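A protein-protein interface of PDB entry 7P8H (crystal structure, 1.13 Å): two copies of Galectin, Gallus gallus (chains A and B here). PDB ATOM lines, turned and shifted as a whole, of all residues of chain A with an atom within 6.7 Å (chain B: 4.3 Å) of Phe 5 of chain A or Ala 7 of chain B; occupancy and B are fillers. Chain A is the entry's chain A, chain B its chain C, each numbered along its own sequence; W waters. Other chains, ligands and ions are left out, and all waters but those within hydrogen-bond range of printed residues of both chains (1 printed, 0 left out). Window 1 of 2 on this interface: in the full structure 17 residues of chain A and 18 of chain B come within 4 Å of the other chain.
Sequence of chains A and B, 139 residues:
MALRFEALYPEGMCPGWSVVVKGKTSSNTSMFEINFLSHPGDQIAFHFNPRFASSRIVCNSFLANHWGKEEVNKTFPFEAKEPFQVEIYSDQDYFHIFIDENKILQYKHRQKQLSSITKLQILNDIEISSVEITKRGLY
Phe 5 of chain A touches Ala 7 of chain B, and with the chains exchanged Ala 7 of chain A touches Phe 5 of chain B.
Phe 5 of chain A touches Leu 8 of chain B, and with the chains exchanged Leu 8 of chain A touches Phe 5 of chain B.
Glu 6 of chain A touches Ala 7 of chain B, and with the chains exchanged Ala 7 of chain A touches Glu 6 of chain B.
Glu 6 of chain A touches Leu 8 of chain B, and with the chains exchanged Leu 8 of chain A touches Glu 6 of chain B.
Water W1 lies within hydrogen-bond range of OE2 of Glu 6 of chain A (2.9 Å) and OE2 of Glu 6 of chain B (2.9 Å).
Among the printed residues, merely in contact across the chains: Glu 6 of chain A with Ala 7 of chain B (3.1 Å), Ala 7 of chain A with Glu 6 of chain B (3.2 Å), Phe 5 of chain A with Leu 8 of chain B (3.2 Å), Leu 8 of chain A with Phe 5 of chain B (3.2 Å), Leu 3 of chain A with Leu 8 of chain B (3.9 Å), Ala 7 of chain A with Phe 5 of chain B (3.9 Å) and Phe 5 of chain A with Ala 7 of chain B (3.9 Å).
Of chain A, only Phe 5 and Glu 6 come within 4 Å of Ala 7 of chain B.
Of the printed residues of chain B, Val 131 of chain A touches Ile 133.
Printed residues of chain A within 4 Å of Glu 6 of chain B: Ala 7 (3.2 Å) and Leu 8 (2.8 Å).
Of the printed residues of chain A, Leu 8 of chain B touches Leu 3, Phe 5 and Glu 6.
Printed residues of chain B within 4 Å of Leu 3 of chain A: Leu 8 (3.9 Å).
Of the printed residues of chain B, Leu 8 of chain A touches Phe 5 and Glu 6.
Leu 123 of chain A touches none of the printed residues of chain B.
Leu 120 of chain B touches none of the printed residues of chain A.
The nearest residue of chain A that does not touch Ala 7 of chain B is Ala 7 of chain A (4.3 Å).
N of Ile 122 of chain A lies within hydrogen-bond range of O of Phe 5 of chain A (2.9 Å).
OE1 of Glu 6 of chain A is in hydrogen-bond range of NE2 of Gln 121 of chain A, 2.8 Å away.
The backbone carbonyl oxygen (O) of Ala 7 of chain A lies within hydrogen-bond range of the backbone NH (N) of Leu 120 of chain A (2.9 Å).
The backbone NH of Leu 120 of chain B lies within hydrogen-bond range of the backbone carbonyl oxygen of Ala 7 of chain B.
Of the 9 printed residues of chain B, 5 touch a printed residue of chain A.
Printed residues of chain B that touch a printed residue of chain A: Phe 5, Glu 6, Ala 7, Leu 8 and Ile 133.
Along chain B the printed residues that touch a printed residue of chain A span positions 5 to 133.
Printed residues of chain A that touch a printed residue of chain B: Leu 3, Phe 5, Glu 6, Ala 7, Leu 8 and Val 131.
Hydrophobic or aromatic side chains of chain A that line the printed part of chain B: Leu 3, Phe 5 and Ala 7.
Along chain A the printed residues that touch a printed residue of chain B span positions 3 to 131.
The backbone carbonyl oxygen of Glu 6 of chain A sits at hydrogen-bond distance from the backbone NH of Leu 8 of chain B, at 2.8 Å.
The backbone carbonyl oxygen (O) of Glu 6 of chain B sits at hydrogen-bond distance from the backbone NH (N) of Leu 8 of chain A (2.8 Å).
The backbone carbonyl oxygen of Val 131 of chain A lies within hydrogen-bond range of the backbone NH of Ile 133 of chain B, 2.9 Å away.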
ATOM      1  N   ALA A   2       1.509 -21.374 -20.430  1.00  0.00           N
ATOM      2  CA  ALA A   2       1.692 -21.227 -21.869  1.00  0.00           C
ATOM      3  C   ALA A   2       3.042 -20.600 -22.155  1.00  0.00           C
ATOM      4  O   ALA A   2       3.372 -19.539 -21.639  1.00  0.00           O
ATOM      5  CB  ALA A   2       0.587 -20.382 -22.467  1.00  0.00           C
ATOM      6  N   LEU A   3       3.801 -21.261 -23.020  1.00  0.00           N
ATOM      7  CA  LEU A   3       5.102 -20.774 -23.443  1.00  0.00           C
ATOM      8  C   LEU A   3       4.901 -19.667 -24.462  1.00  0.00           C
ATOM      9  O   LEU A   3       4.266 -19.882 -25.500  1.00  0.00           O
ATOM     10  CB  LEU A   3       5.880 -21.916 -24.073  1.00  0.00           C
ATOM     11  CG  LEU A   3       7.253 -21.555 -24.630  1.00  0.00           C
ATOM     12  CD1 LEU A   3       8.206 -21.150 -23.534  1.00  0.00           C
ATOM     13  CD2 LEU A   3       7.791 -22.740 -25.412  1.00  0.00           C
ATOM     14  N   ARG A   4       5.403 -18.478 -24.154  1.00  0.00           N
ATOM     15  CA  ARG A   4       5.330 -17.352 -25.071  1.00  0.00           C
ATOM     16  C   ARG A   4       6.587 -17.175 -25.903  1.00  0.00           C
ATOM     17  O   ARG A   4       6.495 -16.742 -27.054  1.00  0.00           O
ATOM     18  CB  ARG A   4       5.060 -16.057 -24.294  1.00  0.00           C
ATOM     19  CG  ARG A   4       3.834 -16.114 -23.399  1.00  0.00           C
ATOM     20  CD  ARG A   4       2.618 -16.459 -24.205  1.00  0.00           C
ATOM     21  NE  ARG A   4       1.426 -16.508 -23.375  1.00  0.00           N
ATOM     22  CZ  ARG A   4       0.254 -16.957 -23.790  1.00  0.00           C
ATOM     23  NH1 ARG A   4       0.092 -17.423 -25.013  1.00  0.00           N
ATOM     24  NH2 ARG A   4      -0.774 -16.942 -22.954  1.00  0.00           N
ATOM     25  N   PHE A   5       7.748 -17.509 -25.359  1.00  0.00           N
ATOM     26  CA  PHE A   5       9.009 -17.305 -26.056  1.00  0.00           C
ATOM     27  C   PHE A   5      10.058 -18.177 -25.394  1.00  0.00           C
ATOM     28  O   PHE A   5      10.108 -18.275 -24.168  1.00  0.00           O
ATOM     29  CB  PHE A   5       9.438 -15.837 -25.965  1.00  0.00           C
ATOM     30  CG  PHE A   5      10.739 -15.522 -26.650  1.00  0.00           C
ATOM     31  CD1 PHE A   5      11.943 -15.601 -25.971  1.00  0.00           C
ATOM     32  CD2 PHE A   5      10.756 -15.116 -27.964  1.00  0.00           C
ATOM     33  CE1 PHE A   5      13.139 -15.289 -26.601  1.00  0.00           C
ATOM     34  CE2 PHE A   5      11.942 -14.810 -28.588  1.00  0.00           C
ATOM     35  CZ  PHE A   5      13.130 -14.908 -27.906  1.00  0.00           C
ATOM     36  N   GLU A   6      10.912 -18.773 -26.203  1.00  0.00           N
ATOM     37  CA  GLU A   6      12.075 -19.479 -25.700  1.00  0.00           C
ATOM     38  C   GLU A   6      13.272 -19.126 -26.567  1.00  0.00           C
ATOM     39  O   GLU A   6      13.133 -18.963 -27.781  1.00  0.00           O
ATOM     40  CB  GLU A   6      11.843 -20.995 -25.760  1.00  0.00           C
ATOM     41  CG  GLU A   6      13.036 -21.861 -25.453  1.00  0.00           C
ATOM     42  CD  GLU A   6      12.694 -23.317 -25.644  1.00  0.00           C
ATOM     43  OE1 GLU A   6      11.971 -23.852 -24.788  1.00  0.00           O
ATOM     44  OE2 GLU A   6      13.104 -23.907 -26.667  1.00  0.00           O
ATOM     45  N   ALA A   7      14.438 -18.995 -25.945  1.00  0.00           N
ATOM     46  CA  ALA A   7      15.687 -18.864 -26.674  1.00  0.00           C
ATOM     47  C   ALA A   7      16.704 -19.838 -26.104  1.00  0.00           C
ATOM     48  O   ALA A   7      16.748 -20.079 -24.894  1.00  0.00           O
ATOM     49  CB  ALA A   7      16.222 -17.437 -26.595  1.00  0.00           C
ATOM     50  N   LEU A   8      17.525 -20.388 -26.988  1.00  0.00           N
ATOM     51  CA  LEU A   8      18.596 -21.304 -26.646  1.00  0.00           C
ATOM     52  C   LEU A   8      19.885 -20.758 -27.249  1.00  0.00           C
ATOM     53  O   LEU A   8      19.941 -20.458 -28.454  1.00  0.00           O
ATOM     54  CB  LEU A   8      18.292 -22.687 -27.211  1.00  0.00           C
ATOM     55  CG  LEU A   8      19.372 -23.748 -27.087  1.00  0.00           C
ATOM     56  CD1 LEU A   8      19.623 -24.073 -25.632  1.00  0.00           C
ATOM     57  CD2 LEU A   8      18.992 -25.010 -27.884  1.00  0.00           C
ATOM     58  N   LEU A 120      16.419 -19.531 -22.083  1.00  0.00           N
ATOM     59  CA  LEU A 120      15.520 -18.517 -21.569  1.00  0.00           C
ATOM     60  C   LEU A 120      14.108 -18.936 -21.951  1.00  0.00           C
ATOM     61  O   LEU A 120      13.860 -19.293 -23.110  1.00  0.00           O
ATOM     62  CB  LEU A 120      15.851 -17.183 -22.248  1.00  0.00           C
ATOM     63  CG  LEU A 120      14.975 -16.003 -21.857  1.00  0.00           C
ATOM     64  CD1 LEU A 120      15.296 -15.523 -20.434  1.00  0.00           C
ATOM     65  CD2 LEU A 120      15.141 -14.887 -22.882  1.00  0.00           C
ATOM     66  N   GLN A 121      13.180 -18.892 -20.992  1.00  0.00           N
ATOM     67  CA  GLN A 121      11.772 -19.139 -21.264  1.00  0.00           C
ATOM     68  C   GLN A 121      10.929 -18.033 -20.654  1.00  0.00           C
ATOM     69  O   GLN A 121      11.176 -17.590 -19.530  1.00  0.00           O
ATOM     70  CB  GLN A 121      11.288 -20.509 -20.738  1.00  0.00           C
ATOM     71  CG  GLN A 121      11.807 -21.700 -21.531  1.00  0.00           C
ATOM     72  CD  GLN A 121      11.088 -23.008 -21.217  1.00  0.00           C
ATOM     73  OE1 GLN A 121      10.527 -23.184 -20.133  1.00  0.00           O
ATOM     74  NE2 GLN A 121      11.114 -23.939 -22.174  1.00  0.00           N
ATOM     75  N   ILE A 122       9.924 -17.592 -21.405  1.00  0.00           N
ATOM     76  CA  ILE A 122       8.983 -16.566 -20.971  1.00  0.00           C
ATOM     77  C   ILE A 122       7.600 -17.194 -21.086  1.00  0.00           C
ATOM     78  O   ILE A 122       7.204 -17.645 -22.172  1.00  0.00           O
ATOM     79  CB  ILE A 122       9.100 -15.296 -21.828  1.00  0.00           C
ATOM     80  CG1 ILE A 122      10.546 -14.784 -21.846  1.00  0.00           C
ATOM     81  CG2 ILE A 122       8.147 -14.249 -21.293  1.00  0.00           C
ATOM     82  CD1 ILE A 122      10.782 -13.607 -22.778  1.00  0.00           C
ATOM     83  N   LEU A 123       6.872 -17.233 -19.966  1.00  0.00           N
ATOM     84  CA  LEU A 123       5.609 -17.944 -19.894  1.00  0.00           C
ATOM     85  C   LEU A 123       4.491 -17.069 -19.341  1.00  0.00           C
ATOM     86  O   LEU A 123       4.716 -16.144 -18.552  1.00  0.00           O
ATOM     87  CB  LEU A 123       5.734 -19.185 -19.022  1.00  0.00           C
ATOM     88  CG  LEU A 123       6.797 -20.166 -19.521  1.00  0.00           C
ATOM     89  CD1 LEU A 123       8.028 -20.152 -18.614  1.00  0.00           C
ATOM     90  CD2 LEU A 123       6.228 -21.570 -19.657  1.00  0.00           C
ATOM     91  N   ILE A 128       4.400 -10.155 -25.736  1.00  0.00           N
ATOM     92  CA  ILE A 128       5.767  -9.710 -25.975  1.00  0.00           C
ATOM     93  C   ILE A 128       5.809  -8.792 -27.183  1.00  0.00           C
ATOM     94  O   ILE A 128       5.251  -9.112 -28.231  1.00  0.00           O
ATOM     95  CB  ILE A 128       6.666 -10.925 -26.201  1.00  0.00           C
ATOM     96  CG1 ILE A 128       6.786 -11.733 -24.905  1.00  0.00           C
ATOM     97  CG2 ILE A 128       8.038 -10.507 -26.702  1.00  0.00           C
ATOM     98  CD1 ILE A 128       7.456 -13.079 -25.090  1.00  0.00           C
ATOM     99  N   VAL A 131      12.263  -9.106 -27.522  1.00  0.00           N
ATOM    100  CA  VAL A 131      13.269  -9.747 -26.689  1.00  0.00           C
ATOM    101  C   VAL A 131      14.635  -9.480 -27.315  1.00  0.00           C
ATOM    102  O   VAL A 131      14.848  -9.792 -28.494  1.00  0.00           O
ATOM    103  CB  VAL A 131      13.060 -11.265 -26.533  1.00  0.00           C
ATOM    104  CG1 VAL A 131      14.122 -11.841 -25.629  1.00  0.00           C
ATOM    105  CG2 VAL A 131      11.664 -11.570 -25.997  1.00  0.00           C
ATOM    106  N   GLU A 132      15.556  -8.936 -26.531  1.00  0.00           N
ATOM    107  CA  GLU A 132      16.904  -8.681 -26.998  1.00  0.00           C
ATOM    108  C   GLU A 132      17.889  -9.326 -26.045  1.00  0.00           C
ATOM    109  O   GLU A 132      17.815  -9.124 -24.833  1.00  0.00           O
ATOM    110  CB  GLU A 132      17.143  -7.193 -27.076  1.00  0.00           C
ATOM    111  CG  GLU A 132      18.485  -6.769 -27.554  1.00  0.00           C
ATOM    112  CD  GLU A 132      18.505  -5.285 -27.543  1.00  0.00           C
ATOM    113  OE1 GLU A 132      18.004  -4.701 -28.524  1.00  0.00           O
ATOM    114  OE2 GLU A 132      18.891  -4.714 -26.503  1.00  0.00           O
ATOM    115  N   ILE A 133      18.797 -10.106 -26.600  1.00  0.00           N
ATOM    116  CA  ILE A 133      19.783 -10.853 -25.838  1.00  0.00           C
ATOM    117  C   ILE A 133      21.159 -10.403 -26.322  1.00  0.00           C
ATOM    118  O   ILE A 133      21.485 -10.571 -27.500  1.00  0.00           O
ATOM    119  CB  ILE A 133      19.565 -12.364 -26.043  1.00  0.00           C
ATOM    120  CG1 ILE A 133      18.160 -12.753 -25.556  1.00  0.00           C
ATOM    121  CG2 ILE A 133      20.651 -13.168 -25.365  1.00  0.00           C
ATOM    122  CD1 ILE A 133      17.749 -14.159 -25.891  1.00  0.00           C
ATOM    123  N   PHE B   5      22.177 -20.335 -32.054  1.00  0.00           N
ATOM    124  CA  PHE B   5      21.078 -19.662 -31.384  1.00  0.00           C
ATOM    125  C   PHE B   5      19.778 -20.168 -31.988  1.00  0.00           C
ATOM    126  O   PHE B   5      19.671 -20.327 -33.210  1.00  0.00           O
ATOM    127  CB  PHE B   5      21.188 -18.143 -31.577  1.00  0.00           C
ATOM    128  CG  PHE B   5      20.093 -17.366 -30.922  1.00  0.00           C
ATOM    129  CD1 PHE B   5      20.219 -16.922 -29.615  1.00  0.00           C
ATOM    130  CD2 PHE B   5      18.941 -17.049 -31.622  1.00  0.00           C
ATOM    131  CE1 PHE B   5      19.206 -16.192 -29.020  1.00  0.00           C
ATOM    132  CE2 PHE B   5      17.923 -16.322 -31.028  1.00  0.00           C
ATOM    133  CZ  PHE B   5      18.057 -15.898 -29.723  1.00  0.00           C
ATOM    134  N   GLU B   6      18.784 -20.389 -31.137  1.00  0.00           N
ATOM    135  CA  GLU B   6      17.444 -20.692 -31.601  1.00  0.00           C
ATOM    136  C   GLU B   6      16.450 -19.900 -30.772  1.00  0.00           C
ATOM    137  O   GLU B   6      16.651 -19.700 -29.568  1.00  0.00           O
ATOM    138  CB  GLU B   6      17.136 -22.192 -31.462  1.00  0.00           C
ATOM    139  CG  GLU B   6      15.716 -22.585 -31.829  1.00  0.00           C
ATOM    140  CD  GLU B   6      15.426 -24.015 -31.465  1.00  0.00           C
ATOM    141  OE1 GLU B   6      15.983 -24.905 -32.126  1.00  0.00           O
ATOM    142  OE2 GLU B   6      14.664 -24.254 -30.503  1.00  0.00           O
ATOM    143  N   ALA B   7      15.383 -19.445 -31.416  1.00  0.00           N
ATOM    144  CA  ALA B   7      14.288 -18.819 -30.700  1.00  0.00           C
ATOM    145  C   ALA B   7      12.978 -19.376 -31.232  1.00  0.00           C
ATOM    146  O   ALA B   7      12.835 -19.682 -32.420  1.00  0.00           O
ATOM    147  CB  ALA B   7      14.279 -17.295 -30.834  1.00  0.00           C
ATOM    148  N   LEU B   8      12.024 -19.497 -30.317  1.00  0.00           N
ATOM    149  CA  LEU B   8      10.683 -19.971 -30.605  1.00  0.00           C
ATOM    150  C   LEU B   8       9.689 -18.955 -30.071  1.00  0.00           C
ATOM    151  O   LEU B   8       9.761 -18.562 -28.900  1.00  0.00           O
ATOM    152  CB  LEU B   8      10.464 -21.313 -29.906  1.00  0.00           C
ATOM    153  CG  LEU B   8       9.103 -21.970 -30.035  1.00  0.00           C
ATOM    154  CD1 LEU B   8       8.816 -22.362 -31.485  1.00  0.00           C
ATOM    155  CD2 LEU B   8       9.038 -23.184 -29.116  1.00  0.00           C
ATOM    156  N   MET B  13       6.001 -15.416 -35.571  1.00  0.00           N
ATOM    157  CA  MET B  13       6.834 -14.217 -35.650  1.00  0.00           C
ATOM    158  C   MET B  13       6.913 -13.691 -37.078  1.00  0.00           C
ATOM    159  O   MET B  13       7.984 -13.285 -37.522  1.00  0.00           O
ATOM    160  CB  MET B  13       8.231 -14.472 -35.060  1.00  0.00           C
ATOM    161  CG  MET B  13       9.079 -15.564 -35.745  1.00  0.00           C
ATOM    162  SD  MET B  13      10.848 -15.579 -35.295  1.00  0.00           S
ATOM    163  CE  MET B  13      10.848 -16.464 -33.746  1.00  0.00           C
ATOM    164  N   THR B 118       7.351 -19.813 -36.644  1.00  0.00           N
ATOM    165  CA  THR B 118       7.483 -19.631 -35.212  1.00  0.00           C
ATOM    166  C   THR B 118       8.910 -19.769 -34.707  1.00  0.00           C
ATOM    167  O   THR B 118       9.143 -19.541 -33.514  1.00  0.00           O
ATOM    168  CB  THR B 118       6.645 -20.686 -34.488  1.00  0.00           C
ATOM    169  OG1 THR B 118       7.124 -21.974 -34.875  1.00  0.00           O
ATOM    170  CG2 THR B 118       5.143 -20.551 -34.793  1.00  0.00           C
ATOM    171  N   LYS B 119       9.855 -20.177 -35.552  1.00  0.00           N
ATOM    172  CA  LYS B 119      11.160 -20.604 -35.090  1.00  0.00           C
ATOM    173  C   LYS B 119      12.257 -19.947 -35.914  1.00  0.00           C
ATOM    174  O   LYS B 119      12.160 -19.845 -37.145  1.00  0.00           O
ATOM    175  CB  LYS B 119      11.235 -22.128 -35.183  1.00  0.00           C
ATOM    176  CG  LYS B 119      12.392 -22.794 -34.513  1.00  0.00           C
ATOM    177  CD  LYS B 119      12.066 -24.284 -34.437  1.00  0.00           C
ATOM    178  CE  LYS B 119      13.108 -25.100 -33.713  1.00  0.00           C
ATOM    179  NZ  LYS B 119      12.733 -26.545 -33.787  1.00  0.00           N
ATOM    180  N   LEU B 120      13.286 -19.486 -35.215  1.00  0.00           N
ATOM    181  CA  LEU B 120      14.458 -18.878 -35.812  1.00  0.00           C
ATOM    182  C   LEU B 120      15.661 -19.702 -35.388  1.00  0.00           C
ATOM    183  O   LEU B 120      15.807 -20.020 -34.202  1.00  0.00           O
ATOM    184  CB  LEU B 120      14.626 -17.465 -35.253  1.00  0.00           C
ATOM    185  CG  LEU B 120      15.900 -16.740 -35.672  1.00  0.00           C
ATOM    186  CD1 LEU B 120      15.777 -16.279 -37.146  1.00  0.00           C
ATOM    187  CD2 LEU B 120      16.177 -15.606 -34.708  1.00  0.00           C
ATOM    188  N   ILE B 133      14.627  -9.666 -31.333  1.00  0.00           N
ATOM    189  CA  ILE B 133      13.429 -10.105 -32.033  1.00  0.00           C
ATOM    190  C   ILE B 133      12.302  -9.180 -31.595  1.00  0.00           C
ATOM    191  O   ILE B 133      11.950  -9.151 -30.411  1.00  0.00           O
ATOM    192  CB  ILE B 133      13.119 -11.574 -31.737  1.00  0.00           C
ATOM    193  CG1 ILE B 133      14.323 -12.423 -32.160  1.00  0.00           C
ATOM    194  CG2 ILE B 133      11.858 -11.982 -32.460  1.00  0.00           C
ATOM    195  CD1 ILE B 133      14.207 -13.887 -31.803  1.00  0.00           C
HETATM  196  O   HOH W   1      14.426 -22.153 -28.492  1.00  0.00           O
